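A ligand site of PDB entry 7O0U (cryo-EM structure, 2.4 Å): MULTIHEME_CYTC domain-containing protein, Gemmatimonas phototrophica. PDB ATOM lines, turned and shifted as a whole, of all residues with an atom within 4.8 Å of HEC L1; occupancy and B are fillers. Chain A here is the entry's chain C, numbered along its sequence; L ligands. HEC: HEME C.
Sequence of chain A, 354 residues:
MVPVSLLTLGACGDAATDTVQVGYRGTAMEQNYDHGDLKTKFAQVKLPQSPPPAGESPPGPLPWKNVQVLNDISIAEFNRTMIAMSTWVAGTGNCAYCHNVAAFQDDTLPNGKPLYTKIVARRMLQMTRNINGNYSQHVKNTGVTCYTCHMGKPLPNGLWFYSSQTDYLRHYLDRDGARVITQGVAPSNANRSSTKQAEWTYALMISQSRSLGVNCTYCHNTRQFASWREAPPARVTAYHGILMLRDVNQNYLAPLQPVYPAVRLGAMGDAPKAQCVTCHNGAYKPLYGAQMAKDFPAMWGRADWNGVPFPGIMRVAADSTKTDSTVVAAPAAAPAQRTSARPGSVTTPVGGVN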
ATOM      1  N   TRP A  64      17.460  -4.806  -7.618  1.00  0.00           N
ATOM      2  CA  TRP A  64      18.611  -4.746  -6.731  1.00  0.00           C
ATOM      3  C   TRP A  64      19.591  -5.902  -6.937  1.00  0.00           C
ATOM      4  O   TRP A  64      19.194  -7.042  -7.152  1.00  0.00           O
ATOM      5  CB  TRP A  64      18.150  -4.739  -5.281  1.00  0.00           C
ATOM      6  CG  TRP A  64      16.987  -3.837  -5.004  1.00  0.00           C
ATOM      7  CD1 TRP A  64      15.786  -4.199  -4.469  1.00  0.00           C
ATOM      8  CD2 TRP A  64      16.910  -2.433  -5.225  1.00  0.00           C
ATOM      9  NE1 TRP A  64      14.969  -3.106  -4.347  1.00  0.00           N
ATOM     10  CE2 TRP A  64      15.636  -2.000  -4.810  1.00  0.00           C
ATOM     11  CE3 TRP A  64      17.803  -1.480  -5.740  1.00  0.00           C
ATOM     12  CZ2 TRP A  64      15.222  -0.681  -4.892  1.00  0.00           C
ATOM     13  CZ3 TRP A  64      17.390  -0.160  -5.822  1.00  0.00           C
ATOM     14  CH2 TRP A  64      16.118   0.230  -5.394  1.00  0.00           C
ATOM     15  N   LYS A  65      20.881  -5.575  -6.850  1.00  0.00           N
ATOM     16  CA  LYS A  65      21.964  -6.512  -7.088  1.00  0.00           C
ATOM     17  C   LYS A  65      22.429  -7.213  -5.815  1.00  0.00           C
ATOM     18  O   LYS A  65      22.828  -8.378  -5.877  1.00  0.00           O
ATOM     19  CB  LYS A  65      23.140  -5.777  -7.738  1.00  0.00           C
ATOM     20  CG  LYS A  65      22.815  -5.309  -9.147  1.00  0.00           C
ATOM     21  CD  LYS A  65      23.812  -4.295  -9.672  1.00  0.00           C
ATOM     22  CE  LYS A  65      23.317  -3.700 -10.985  1.00  0.00           C
ATOM     23  NZ  LYS A  65      24.193  -2.610 -11.483  1.00  0.00           N
ATOM     24  N   ASN A  66      22.387  -6.533  -4.673  1.00  0.00           N
ATOM     25  CA  ASN A  66      22.984  -7.013  -3.436  1.00  0.00           C
ATOM     26  C   ASN A  66      22.115  -6.602  -2.253  1.00  0.00           C
ATOM     27  O   ASN A  66      22.578  -6.031  -1.263  1.00  0.00           O
ATOM     28  CB  ASN A  66      24.417  -6.497  -3.297  1.00  0.00           C
ATOM     29  CG  ASN A  66      25.147  -7.075  -2.098  1.00  0.00           C
ATOM     30  OD1 ASN A  66      24.822  -8.163  -1.634  1.00  0.00           O
ATOM     31  ND2 ASN A  66      26.151  -6.353  -1.617  1.00  0.00           N
ATOM     32  N   VAL A  67      20.813  -6.869  -2.362  1.00  0.00           N
ATOM     33  CA  VAL A  67      19.851  -6.645  -1.295  1.00  0.00           C
ATOM     34  C   VAL A  67      19.433  -7.991  -0.722  1.00  0.00           C
ATOM     35  O   VAL A  67      18.911  -8.854  -1.438  1.00  0.00           O
ATOM     36  CB  VAL A  67      18.636  -5.838  -1.778  1.00  0.00           C
ATOM     37  CG1 VAL A  67      17.504  -5.924  -0.772  1.00  0.00           C
ATOM     38  CG2 VAL A  67      19.035  -4.390  -1.946  1.00  0.00           C
ATOM     39  N   GLN A  68      19.664  -8.171   0.579  1.00  0.00           N
ATOM     40  CA  GLN A  68      19.548  -9.457   1.250  1.00  0.00           C
ATOM     41  C   GLN A  68      18.464  -9.495   2.305  1.00  0.00           C
ATOM     42  O   GLN A  68      18.014 -10.582   2.677  1.00  0.00           O
ATOM     43  CB  GLN A  68      20.889  -9.837   1.882  1.00  0.00           C
ATOM     44  CG  GLN A  68      22.033  -9.919   0.878  1.00  0.00           C
ATOM     45  CD  GLN A  68      23.359 -10.304   1.503  1.00  0.00           C
ATOM     46  OE1 GLN A  68      23.396 -10.965   2.542  1.00  0.00           O
ATOM     47  NE2 GLN A  68      24.447  -9.888   0.880  1.00  0.00           N
ATOM     48  N   VAL A  69      18.023  -8.335   2.789  1.00  0.00           N
ATOM     49  CA  VAL A  69      17.003  -8.231   3.825  1.00  0.00           C
ATOM     50  C   VAL A  69      15.727  -7.602   3.265  1.00  0.00           C
ATOM     51  O   VAL A  69      14.640  -8.169   3.384  1.00  0.00           O
ATOM     52  CB  VAL A  69      17.523  -7.439   5.043  1.00  0.00           C
ATOM     53  CG1 VAL A  69      16.469  -7.387   6.136  1.00  0.00           C
ATOM     54  CG2 VAL A  69      18.807  -8.057   5.562  1.00  0.00           C
ATOM     55  N   LEU A  70      15.855  -6.421   2.664  1.00  0.00           N
ATOM     56  CA  LEU A  70      14.730  -5.599   2.221  1.00  0.00           C
ATOM     57  C   LEU A  70      14.123  -6.062   0.896  1.00  0.00           C
ATOM     58  O   LEU A  70      13.410  -5.287   0.253  1.00  0.00           O
ATOM     59  CB  LEU A  70      15.171  -4.140   2.112  1.00  0.00           C
ATOM     60  CG  LEU A  70      15.654  -3.496   3.405  1.00  0.00           C
ATOM     61  CD1 LEU A  70      16.017  -2.037   3.177  1.00  0.00           C
ATOM     62  CD2 LEU A  70      14.590  -3.612   4.491  1.00  0.00           C
ATOM     63  N   PHE A  78      11.468   0.967  -0.574  1.00  0.00           N
ATOM     64  CA  PHE A  78      12.907   0.809  -0.378  1.00  0.00           C
ATOM     65  C   PHE A  78      13.631   2.150  -0.356  1.00  0.00           C
ATOM     66  O   PHE A  78      14.381   2.442   0.579  1.00  0.00           O
ATOM     67  CB  PHE A  78      13.460  -0.104  -1.474  1.00  0.00           C
ATOM     68  CG  PHE A  78      14.901  -0.473  -1.308  1.00  0.00           C
ATOM     69  CD1 PHE A  78      15.909   0.417  -1.649  1.00  0.00           C
ATOM     70  CD2 PHE A  78      15.261  -1.720  -0.824  1.00  0.00           C
ATOM     71  CE1 PHE A  78      17.233   0.072  -1.508  1.00  0.00           C
ATOM     72  CE2 PHE A  78      16.578  -2.072  -0.678  1.00  0.00           C
ATOM     73  CZ  PHE A  78      17.579  -1.175  -1.022  1.00  0.00           C
ATOM     74  N   ASN A  79      13.426   2.969  -1.388  1.00  0.00           N
ATOM     75  CA  ASN A  79      14.091   4.265  -1.450  1.00  0.00           C
ATOM     76  C   ASN A  79      13.669   5.157  -0.285  1.00  0.00           C
ATOM     77  O   ASN A  79      14.489   5.896   0.274  1.00  0.00           O
ATOM     78  CB  ASN A  79      13.785   4.946  -2.773  1.00  0.00           C
ATOM     79  CG  ASN A  79      14.714   4.493  -3.880  1.00  0.00           C
ATOM     80  OD1 ASN A  79      15.882   4.865  -3.910  1.00  0.00           O
ATOM     81  ND2 ASN A  79      14.195   3.681  -4.798  1.00  0.00           N
ATOM     82  N   MET A  82      15.672   4.099   2.751  1.00  0.00           N
ATOM     83  CA  MET A  82      17.044   4.624   2.741  1.00  0.00           C
ATOM     84  C   MET A  82      17.104   6.087   3.141  1.00  0.00           C
ATOM     85  O   MET A  82      18.042   6.513   3.832  1.00  0.00           O
ATOM     86  CB  MET A  82      17.662   4.427   1.359  1.00  0.00           C
ATOM     87  CG  MET A  82      17.891   2.978   0.991  1.00  0.00           C
ATOM     88  SD  MET A  82      19.098   2.188   2.076  1.00  0.00           S
ATOM     89  CE  MET A  82      18.588   0.479   1.896  1.00  0.00           C
ATOM     90  N   ILE A  83      16.120   6.890   2.741  1.00  0.00           N
ATOM     91  CA  ILE A  83      16.053   8.281   3.195  1.00  0.00           C
ATOM     92  C   ILE A  83      15.861   8.338   4.705  1.00  0.00           C
ATOM     93  O   ILE A  83      16.495   9.148   5.393  1.00  0.00           O
ATOM     94  CB  ILE A  83      14.930   9.024   2.450  1.00  0.00           C
ATOM     95  CG1 ILE A  83      15.284   9.152   0.969  1.00  0.00           C
ATOM     96  CG2 ILE A  83      14.698  10.390   3.062  1.00  0.00           C
ATOM     97  CD1 ILE A  83      14.089   9.387   0.081  1.00  0.00           C
ATOM     98  N   MET A  85      16.701   5.864   6.942  1.00  0.00           N
ATOM     99  CA  MET A  85      17.918   5.343   7.575  1.00  0.00           C
ATOM    100  C   MET A  85      19.027   6.389   7.643  1.00  0.00           C
ATOM    101  O   MET A  85      19.680   6.535   8.682  1.00  0.00           O
ATOM    102  CB  MET A  85      18.394   4.095   6.825  1.00  0.00           C
ATOM    103  CG  MET A  85      17.544   2.867   7.087  1.00  0.00           C
ATOM    104  SD  MET A  85      17.930   1.471   6.027  1.00  0.00           S
ATOM    105  CE  MET A  85      19.702   1.366   6.218  1.00  0.00           C
ATOM    106  N   SER A  86      19.259   7.118   6.549  1.00  0.00           N
ATOM    107  CA  SER A  86      20.243   8.194   6.590  1.00  0.00           C
ATOM    108  C   SER A  86      19.860   9.271   7.600  1.00  0.00           C
ATOM    109  O   SER A  86      20.695   9.725   8.388  1.00  0.00           O
ATOM    110  CB  SER A  86      20.414   8.798   5.192  1.00  0.00           C
ATOM    111  OG  SER A  86      19.164   9.225   4.674  1.00  0.00           O
ATOM    112  N   VAL A  89      20.283   7.522  11.303  1.00  0.00           N
ATOM    113  CA  VAL A  89      21.622   7.145  11.749  1.00  0.00           C
ATOM    114  C   VAL A  89      22.653   8.227  11.471  1.00  0.00           C
ATOM    115  O   VAL A  89      23.549   8.452  12.290  1.00  0.00           O
ATOM    116  CB  VAL A  89      22.035   5.810  11.102  1.00  0.00           C
ATOM    117  CG1 VAL A  89      23.387   5.349  11.629  1.00  0.00           C
ATOM    118  CG2 VAL A  89      20.980   4.741  11.364  1.00  0.00           C
ATOM    119  N   ALA A  90      22.547   8.925  10.337  1.00  0.00           N
ATOM    120  CA  ALA A  90      23.697   9.611   9.763  1.00  0.00           C
ATOM    121  C   ALA A  90      23.435  11.053   9.365  1.00  0.00           C
ATOM    122  O   ALA A  90      24.320  11.690   8.765  1.00  0.00           O
ATOM    123  CB  ALA A  90      24.218   8.825   8.551  1.00  0.00           C
ATOM    124  N   GLY A  93      20.087  12.650   3.911  1.00  0.00           N
ATOM    125  CA  GLY A  93      20.806  12.685   2.653  1.00  0.00           C
ATOM    126  C   GLY A  93      22.243  12.224   2.699  1.00  0.00           C
ATOM    127  O   GLY A  93      22.929  12.300   1.663  1.00  0.00           O
ATOM    128  N   ASN A  94      22.727  11.741   3.834  1.00  0.00           N
ATOM    129  CA  ASN A  94      24.121  11.313   4.004  1.00  0.00           C
ATOM    130  C   ASN A  94      24.325   9.850   3.600  1.00  0.00           C
ATOM    131  O   ASN A  94      24.867   9.059   4.361  1.00  0.00           O
ATOM    132  CB  ASN A  94      24.548  11.558   5.436  1.00  0.00           C
ATOM    133  CG  ASN A  94      26.047  11.473   5.621  1.00  0.00           C
ATOM    134  OD1 ASN A  94      26.808  11.467   4.647  1.00  0.00           O
ATOM    135  ND2 ASN A  94      26.496  11.430   6.868  1.00  0.00           N
ATOM    136  N   CYS A  95      23.879   9.476   2.392  1.00  0.00           N
ATOM    137  CA  CYS A  95      24.084   8.114   1.907  1.00  0.00           C
ATOM    138  C   CYS A  95      25.562   7.712   1.892  1.00  0.00           C
ATOM    139  O   CYS A  95      25.879   6.524   1.978  1.00  0.00           O
ATOM    140  CB  CYS A  95      23.515   7.968   0.502  1.00  0.00           C
ATOM    141  SG  CYS A  95      21.858   8.641   0.278  1.00  0.00           S
ATOM    142  N   TYR A  97      27.552   7.923   4.247  1.00  0.00           N
ATOM    143  CA  TYR A  97      27.942   7.286   5.502  1.00  0.00           C
ATOM    144  C   TYR A  97      28.071   5.776   5.362  1.00  0.00           C
ATOM    145  O   TYR A  97      28.978   5.169   5.937  1.00  0.00           O
ATOM    146  CB  TYR A  97      26.959   7.639   6.613  1.00  0.00           C
ATOM    147  CG  TYR A  97      27.576   7.459   7.979  1.00  0.00           C
ATOM    148  CD1 TYR A  97      28.470   8.386   8.482  1.00  0.00           C
ATOM    149  CD2 TYR A  97      27.337   6.319   8.729  1.00  0.00           C
ATOM    150  CE1 TYR A  97      29.035   8.236   9.721  1.00  0.00           C
ATOM    151  CE2 TYR A  97      27.924   6.129   9.965  1.00  0.00           C
ATOM    152  CZ  TYR A  97      28.765   7.102  10.459  1.00  0.00           C
ATOM    153  OH  TYR A  97      29.386   6.910  11.670  1.00  0.00           O
ATOM    154  N   CYS A  98      27.168   5.154   4.619  1.00  0.00           N
ATOM    155  CA  CYS A  98      27.216   3.708   4.405  1.00  0.00           C
ATOM    156  C   CYS A  98      27.773   3.280   3.057  1.00  0.00           C
ATOM    157  O   CYS A  98      28.358   2.203   2.961  1.00  0.00           O
ATOM    158  CB  CYS A  98      25.823   3.095   4.582  1.00  0.00           C
ATOM    159  SG  CYS A  98      25.080   3.404   6.202  1.00  0.00           S
ATOM    160  N   HIS A  99      27.611   4.101   2.020  1.00  0.00           N
ATOM    161  CA  HIS A  99      27.784   3.627   0.656  1.00  0.00           C
ATOM    162  C   HIS A  99      29.032   4.191  -0.021  1.00  0.00           C
ATOM    163  O   HIS A  99      29.484   5.293   0.290  1.00  0.00           O
ATOM    164  CB  HIS A  99      26.574   4.014  -0.190  1.00  0.00           C
ATOM    165  CG  HIS A  99      25.347   3.193   0.065  1.00  0.00           C
ATOM    166  ND1 HIS A  99      25.224   1.881  -0.345  1.00  0.00           N
ATOM    167  CD2 HIS A  99      24.180   3.500   0.690  1.00  0.00           C
ATOM    168  CE1 HIS A  99      24.035   1.426   0.022  1.00  0.00           C
ATOM    169  NE2 HIS A  99      23.390   2.387   0.651  1.00  0.00           N
ATOM    170  N   PHE A 104      26.067   1.777  -5.147  1.00  0.00           N
ATOM    171  CA  PHE A 104      25.300   1.433  -3.952  1.00  0.00           C
ATOM    172  C   PHE A 104      25.317  -0.067  -3.659  1.00  0.00           C
ATOM    173  O   PHE A 104      25.226  -0.465  -2.490  1.00  0.00           O
ATOM    174  CB  PHE A 104      23.857   1.923  -4.105  1.00  0.00           C
ATOM    175  CG  PHE A 104      23.738   3.414  -4.118  1.00  0.00           C
ATOM    176  CD1 PHE A 104      23.750   4.131  -2.934  1.00  0.00           C
ATOM    177  CD2 PHE A 104      23.605   4.106  -5.304  1.00  0.00           C
ATOM    178  CE1 PHE A 104      23.638   5.505  -2.926  1.00  0.00           C
ATOM    179  CE2 PHE A 104      23.497   5.476  -5.318  1.00  0.00           C
ATOM    180  CZ  PHE A 104      23.510   6.181  -4.127  1.00  0.00           C
ATOM    181  N   GLN A 105      25.414  -0.909  -4.680  1.00  0.00           N
ATOM    182  CA  GLN A 105      25.477  -2.348  -4.460  1.00  0.00           C
ATOM    183  C   GLN A 105      26.766  -2.813  -3.798  1.00  0.00           C
ATOM    184  O   GLN A 105      26.770  -3.897  -3.208  1.00  0.00           O
ATOM    185  CB  GLN A 105      25.257  -3.106  -5.785  1.00  0.00           C
ATOM    186  CG  GLN A 105      26.430  -3.087  -6.758  1.00  0.00           C
ATOM    187  CD  GLN A 105      26.562  -1.789  -7.528  1.00  0.00           C
ATOM    188  OE1 GLN A 105      25.829  -0.836  -7.278  1.00  0.00           O
ATOM    189  NE2 GLN A 105      27.474  -1.759  -8.480  1.00  0.00           N
ATOM    190  N   THR A 117      30.273   0.065   7.909  1.00  0.00           N
ATOM    191  CA  THR A 117      28.999   0.690   8.262  1.00  0.00           C
ATOM    192  C   THR A 117      27.825   0.074   7.518  1.00  0.00           C
ATOM    193  O   THR A 117      26.739  -0.106   8.100  1.00  0.00           O
ATOM    194  CB  THR A 117      29.102   2.187   7.958  1.00  0.00           C
ATOM    195  OG1 THR A 117      30.260   2.726   8.608  1.00  0.00           O
ATOM    196  CG2 THR A 117      27.883   2.922   8.439  1.00  0.00           C
ATOM    197  N   LYS A 118      27.997  -0.281   6.237  1.00  0.00           N
ATOM    198  CA  LYS A 118      26.941  -0.960   5.506  1.00  0.00           C
ATOM    199  C   LYS A 118      26.717  -2.388   6.014  1.00  0.00           C
ATOM    200  O   LYS A 118      25.580  -2.847   6.101  1.00  0.00           O
ATOM    201  CB  LYS A 118      27.240  -0.959   4.010  1.00  0.00           C
ATOM    202  CG  LYS A 118      26.063  -1.424   3.159  1.00  0.00           C
ATOM    203  CD  LYS A 118      26.370  -1.390   1.678  1.00  0.00           C
ATOM    204  CE  LYS A 118      25.223  -1.964   0.874  1.00  0.00           C
ATOM    205  NZ  LYS A 118      25.620  -2.340  -0.500  1.00  0.00           N
ATOM    206  N   ALA A 121      24.825  -2.021   9.251  1.00  0.00           N
ATOM    207  CA  ALA A 121      23.445  -1.603   9.017  1.00  0.00           C
ATOM    208  C   ALA A 121      22.575  -2.735   8.477  1.00  0.00           C
ATOM    209  O   ALA A 121      21.386  -2.832   8.814  1.00  0.00           O
ATOM    210  CB  ALA A 121      23.416  -0.410   8.057  1.00  0.00           C
ATOM    211  N   ARG A 122      23.136  -3.611   7.635  1.00  0.00           N
ATOM    212  CA  ARG A 122      22.395  -4.793   7.215  1.00  0.00           C
ATOM    213  C   ARG A 122      22.014  -5.674   8.398  1.00  0.00           C
ATOM    214  O   ARG A 122      20.891  -6.195   8.461  1.00  0.00           O
ATOM    215  CB  ARG A 122      23.193  -5.587   6.175  1.00  0.00           C
ATOM    216  CG  ARG A 122      22.406  -6.731   5.553  1.00  0.00           C
ATOM    217  CD  ARG A 122      23.201  -7.470   4.495  1.00  0.00           C
ATOM    218  NE  ARG A 122      23.257  -6.711   3.252  1.00  0.00           N
ATOM    219  CZ  ARG A 122      24.356  -6.527   2.529  1.00  0.00           C
ATOM    220  NH1 ARG A 122      25.551  -6.911   2.959  1.00  0.00           N
ATOM    221  NH2 ARG A 122      24.261  -5.895   1.361  1.00  0.00           N
ATOM    222  N   LEU A 125      19.210  -3.924  10.427  1.00  0.00           N
ATOM    223  CA  LEU A 125      17.884  -4.198   9.874  1.00  0.00           C
ATOM    224  C   LEU A 125      17.329  -5.532  10.374  1.00  0.00           C
ATOM    225  O   LEU A 125      16.180  -5.600  10.818  1.00  0.00           O
ATOM    226  CB  LEU A 125      17.951  -4.174   8.343  1.00  0.00           C
ATOM    227  CG  LEU A 125      18.012  -2.788   7.714  1.00  0.00           C
ATOM    228  CD1 LEU A 125      18.507  -2.878   6.284  1.00  0.00           C
ATOM    229  CD2 LEU A 125      16.635  -2.148   7.746  1.00  0.00           C
HETATM  230 FE   HEC L   1      21.365   2.302   1.274  1.00  0.00          FE
HETATM  231  CHA HEC L   1      21.196  -0.869  -0.063  1.00  0.00           C
HETATM  232  CHB HEC L   1      20.456   3.613  -1.775  1.00  0.00           C
HETATM  233  CHC HEC L   1      21.659   5.496   2.528  1.00  0.00           C
HETATM  234  CHD HEC L   1      22.557   1.072   4.213  1.00  0.00           C
HETATM  235  NA  HEC L   1      20.892   1.518  -0.564  1.00  0.00           N
HETATM  236  C1A HEC L   1      20.920   0.174  -0.914  1.00  0.00           C
HETATM  237  C2A HEC L   1      20.619   0.080  -2.330  1.00  0.00           C
HETATM  238  C3A HEC L   1      20.413   1.315  -2.789  1.00  0.00           C
HETATM  239  C4A HEC L   1      20.586   2.248  -1.696  1.00  0.00           C
HETATM  240  CMA HEC L   1      20.064   1.696  -4.249  1.00  0.00           C
HETATM  241  CAA HEC L   1      20.542  -1.229  -3.138  1.00  0.00           C
HETATM  242  CBA HEC L   1      21.832  -1.479  -3.913  1.00  0.00           C
HETATM  243  CGA HEC L   1      21.730  -2.769  -4.683  1.00  0.00           C
HETATM  244  O1A HEC L   1      22.160  -3.822  -4.154  1.00  0.00           O
HETATM  245  O2A HEC L   1      21.215  -2.750  -5.830  1.00  0.00           O
HETATM  246  NB  HEC L   1      21.193   4.199   0.495  1.00  0.00           N
HETATM  247  C1B HEC L   1      20.638   4.499  -0.737  1.00  0.00           C
HETATM  248  C2B HEC L   1      20.281   5.910  -0.738  1.00  0.00           C
HETATM  249  C3B HEC L   1      20.635   6.429   0.455  1.00  0.00           C
HETATM  250  C4B HEC L   1      21.196   5.351   1.238  1.00  0.00           C
HETATM  251  CMB HEC L   1      19.644   6.592  -1.970  1.00  0.00           C
HETATM  252  CAB HEC L   1      20.502   7.841   1.076  1.00  0.00           C
HETATM  253  CBB HEC L   1      19.327   8.714   0.587  1.00  0.00           C
HETATM  254  NC  HEC L   1      21.969   3.137   3.036  1.00  0.00           N
HETATM  255  C1C HEC L   1      22.052   4.475   3.354  1.00  0.00           C
HETATM  256  C2C HEC L   1      22.406   4.595   4.750  1.00  0.00           C
HETATM  257  C3C HEC L   1      22.852   3.379   5.127  1.00  0.00           C
HETATM  258  C4C HEC L   1      22.453   2.440   4.107  1.00  0.00           C
HETATM  259  CMC HEC L   1      22.813   5.963   5.342  1.00  0.00           C
HETATM  260  CAC HEC L   1      23.427   2.869   6.476  1.00  0.00           C
HETATM  261  CBC HEC L   1      22.928   3.604   7.738  1.00  0.00           C
HETATM  262  ND  HEC L   1      21.865   0.406   1.939  1.00  0.00           N
HETATM  263  C1D HEC L   1      22.201   0.150   3.260  1.00  0.00           C
HETATM  264  C2D HEC L   1      22.124  -1.271   3.507  1.00  0.00           C
HETATM  265  C3D HEC L   1      21.692  -1.886   2.169  1.00  0.00           C
HETATM  266  C4D HEC L   1      21.564  -0.782   1.257  1.00  0.00           C
HETATM  267  CMD HEC L   1      22.396  -2.015   4.823  1.00  0.00           C
HETATM  268  CAD HEC L   1      21.470  -3.383   1.896  1.00  0.00           C
HETATM  269  CBD HEC L   1      20.049  -3.760   2.312  1.00  0.00           C
HETATM  270  CGD HEC L   1      19.882  -5.249   2.203  1.00  0.00           C
HETATM  271  O1D HEC L   1      18.734  -5.740   2.367  1.00  0.00           O
HETATM  272  O2D HEC L   1      20.895  -5.955   1.969  1.00  0.00           O
HETATM  273 FE   HEC L   2      22.332   0.480  15.103  1.00  0.00          FE
HETATM  274  CHA HEC L   2      25.725   0.783  15.555  1.00  0.00           C
HETATM  275  CHB HEC L   2      22.717   1.331  11.791  1.00  0.00           C
HETATM  276  CHC HEC L   2      18.926   0.396  14.655  1.00  0.00           C
HETATM  277  CHD HEC L   2      21.876  -0.044  18.445  1.00  0.00           C
HETATM  278  NA  HEC L   2      23.914   0.960  13.909  1.00  0.00           N
HETATM  279  C1A HEC L   2      25.233   1.035  14.298  1.00  0.00           C
HETATM  280  C2A HEC L   2      26.025   1.415  13.149  1.00  0.00           C
HETATM  281  C3A HEC L   2      25.193   1.567  12.121  1.00  0.00           C
HETATM  282  C4A HEC L   2      23.844   1.280  12.570  1.00  0.00           C
HETATM  283  CMA HEC L   2      25.550   1.969  10.680  1.00  0.00           C
HETATM  284  CAA HEC L   2      27.551   1.622  13.153  1.00  0.00           C
HETATM  285  CBA HEC L   2      27.854   3.036  13.614  1.00  0.00           C
HETATM  286  CGA HEC L   2      29.340   3.297  13.592  1.00  0.00           C
HETATM  287  O1A HEC L   2      29.746   4.402  13.156  1.00  0.00           O
HETATM  288  O2A HEC L   2      30.114   2.397  14.000  1.00  0.00           O
HETATM  289  NB  HEC L   2      21.072   0.878  13.541  1.00  0.00           N
HETATM  290  C1B HEC L   2      21.437   1.076  12.227  1.00  0.00           C
HETATM  291  C2B HEC L   2      20.259   0.934  11.389  1.00  0.00           C
HETATM  292  C3B HEC L   2      19.209   0.701  12.204  1.00  0.00           C
HETATM  293  C4B HEC L   2      19.713   0.638  13.550  1.00  0.00           C
HETATM  294  CMB HEC L   2      20.299   1.109   9.855  1.00  0.00           C
HETATM  295  CAB HEC L   2      17.710   0.447  11.935  1.00  0.00           C
HETATM  296  CBB HEC L   2      17.384  -0.354  10.668  1.00  0.00           C
HETATM  297  NC  HEC L   2      20.710   0.224  16.312  1.00  0.00           N
HETATM  298  C1C HEC L   2      19.383   0.228  15.937  1.00  0.00           C
HETATM  299  C2C HEC L   2      18.582  -0.167  17.073  1.00  0.00           C
HETATM  300  C3C HEC L   2      19.385  -0.081  18.154  1.00  0.00           C
HETATM  301  C4C HEC L   2      20.741   0.029  17.665  1.00  0.00           C
HETATM  302  CMC HEC L   2      17.044  -0.025  17.057  1.00  0.00           C
HETATM  303  CAC HEC L   2      19.116  -0.327  19.658  1.00  0.00           C
HETATM  304  CBC HEC L   2      18.124  -1.467  19.955  1.00  0.00           C
HETATM  305  ND  HEC L   2      23.590   0.434  16.743  1.00  0.00           N
HETATM  306  C1D HEC L   2      23.176   0.071  18.017  1.00  0.00           C
HETATM  307  C2D HEC L   2      24.336  -0.165  18.851  1.00  0.00           C
HETATM  308  C3D HEC L   2      25.537   0.099  17.934  1.00  0.00           C
HETATM  309  C4D HEC L   2      24.975   0.473  16.661  1.00  0.00           C
HETATM  310  CMD HEC L   2      24.354  -0.593  20.326  1.00  0.00           C
HETATM  311  CAD HEC L   2      27.034   0.014  18.280  1.00  0.00           C
HETATM  312  CBD HEC L   2      27.521   1.435  18.487  1.00  0.00           C
HETATM  313  CGD HEC L   2      28.962   1.542  18.050  1.00  0.00           C
HETATM  314  O1D HEC L   2      29.210   1.478  16.826  1.00  0.00           O
HETATM  315  O2D HEC L   2      29.846   1.696  18.933  1.00  0.00           O
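A carbon (CAC) of HEC L1 is covalently linked to the side-chain sulfur (SG) of Cys 98, at 1.8 Å. A carbon (CAB) of HEC L1 is covalently linked to the side-chain sulfur of Cys 95 (1.8 Å). NE2 of His 99 is bound to FE of HEC L1, 2.1 Å away. The side-chain sulfur (SD) of Met 82 is bound to an iron atom (FE) of HEC L1 (2.4 Å). An oxygen (O1D) of HEC L1 lies within hydrogen-bond range of the backbone NH (N) of Val 69. N of Asn 66 is in hydrogen-bond range of O1A of HEC L1, at 2.8 Å. The guanidinium group (NE) of Arg 122 lies within salt-bridge range of an oxygen (O2D) of HEC L1 (2.8 Å). N of Gln 68 lies within hydrogen-bond range of O2D of HEC L1 (2.9 Å). The backbone NH (N) of Leu 70 sits at hydrogen-bond distance from an oxygen (O1D) of HEC L1, 3.0 Å away. An oxygen (O2A) of HEC L1 sits at hydrogen-bond distance from the backbone NH (N) of Lys 65 (3.0 Å). The side-chain hydroxyl (OH) of Tyr 97 is in hydrogen-bond range of an oxygen (O1A) of HEC L2.
A ring nitrogen (ND1) of His 99 sits at hydrogen-bond distance from the backbone carbonyl oxygen (O) of Phe 104. OG of Ser 86 sits at hydrogen-bond distance from O of Met 82 (3.1 Å). The backbone carbonyl oxygen (O) of Asn 66 is in hydrogen-bond range of the guanidinium group (NH2) of Arg 122 (3.1 Å). The side-chain amide oxygen of Asn 66 is in hydrogen-bond range of the side-chain amide nitrogen of Gln 68, 3.1 Å away. ND2 of Asn 66 lies within hydrogen-bond range of O of Gln 105, 3.0 Å away. The side-chain amino group (NZ) of Lys 118 sits at hydrogen-bond distance from the backbone carbonyl oxygen (O) of Phe 104, 2.8 Å away. O of Gln 105 is in hydrogen-bond range of NZ of Lys 118 (3.3 Å). OG of Ser 86 sits at hydrogen-bond distance from O of Ile 83, at 2.8 Å.
CA of Trp 64 touches O2A of HEC L1, at 3.4 Å. Val 67 touches HEC L1 (CG1 to O1D, 3.4 Å). Phe 78 touches HEC L1 (CE1 to C2A, 3.5 Å). Met 85 touches HEC L1 (CE to CHD, 3.5 Å). Ser 86 touches HEC L1. O of Asn 94 touches CMC of HEC L1 (3.8 Å). Phe 104 touches HEC L1 (CD1 to CHB, 3.5 Å). Gln 105 touches HEC L1. Lys 118 touches HEC L1. Ala 121 touches HEC L1. Hydrophobic or aromatic side chains that line HEC L1: Trp 64, Val 67, Val 69, Leu 70, Phe 78, Met 82, Met 85, His 99, Phe 104 and Ala 121. Of the 28 residues printed, 20 come within 4 Å of HEC L1.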
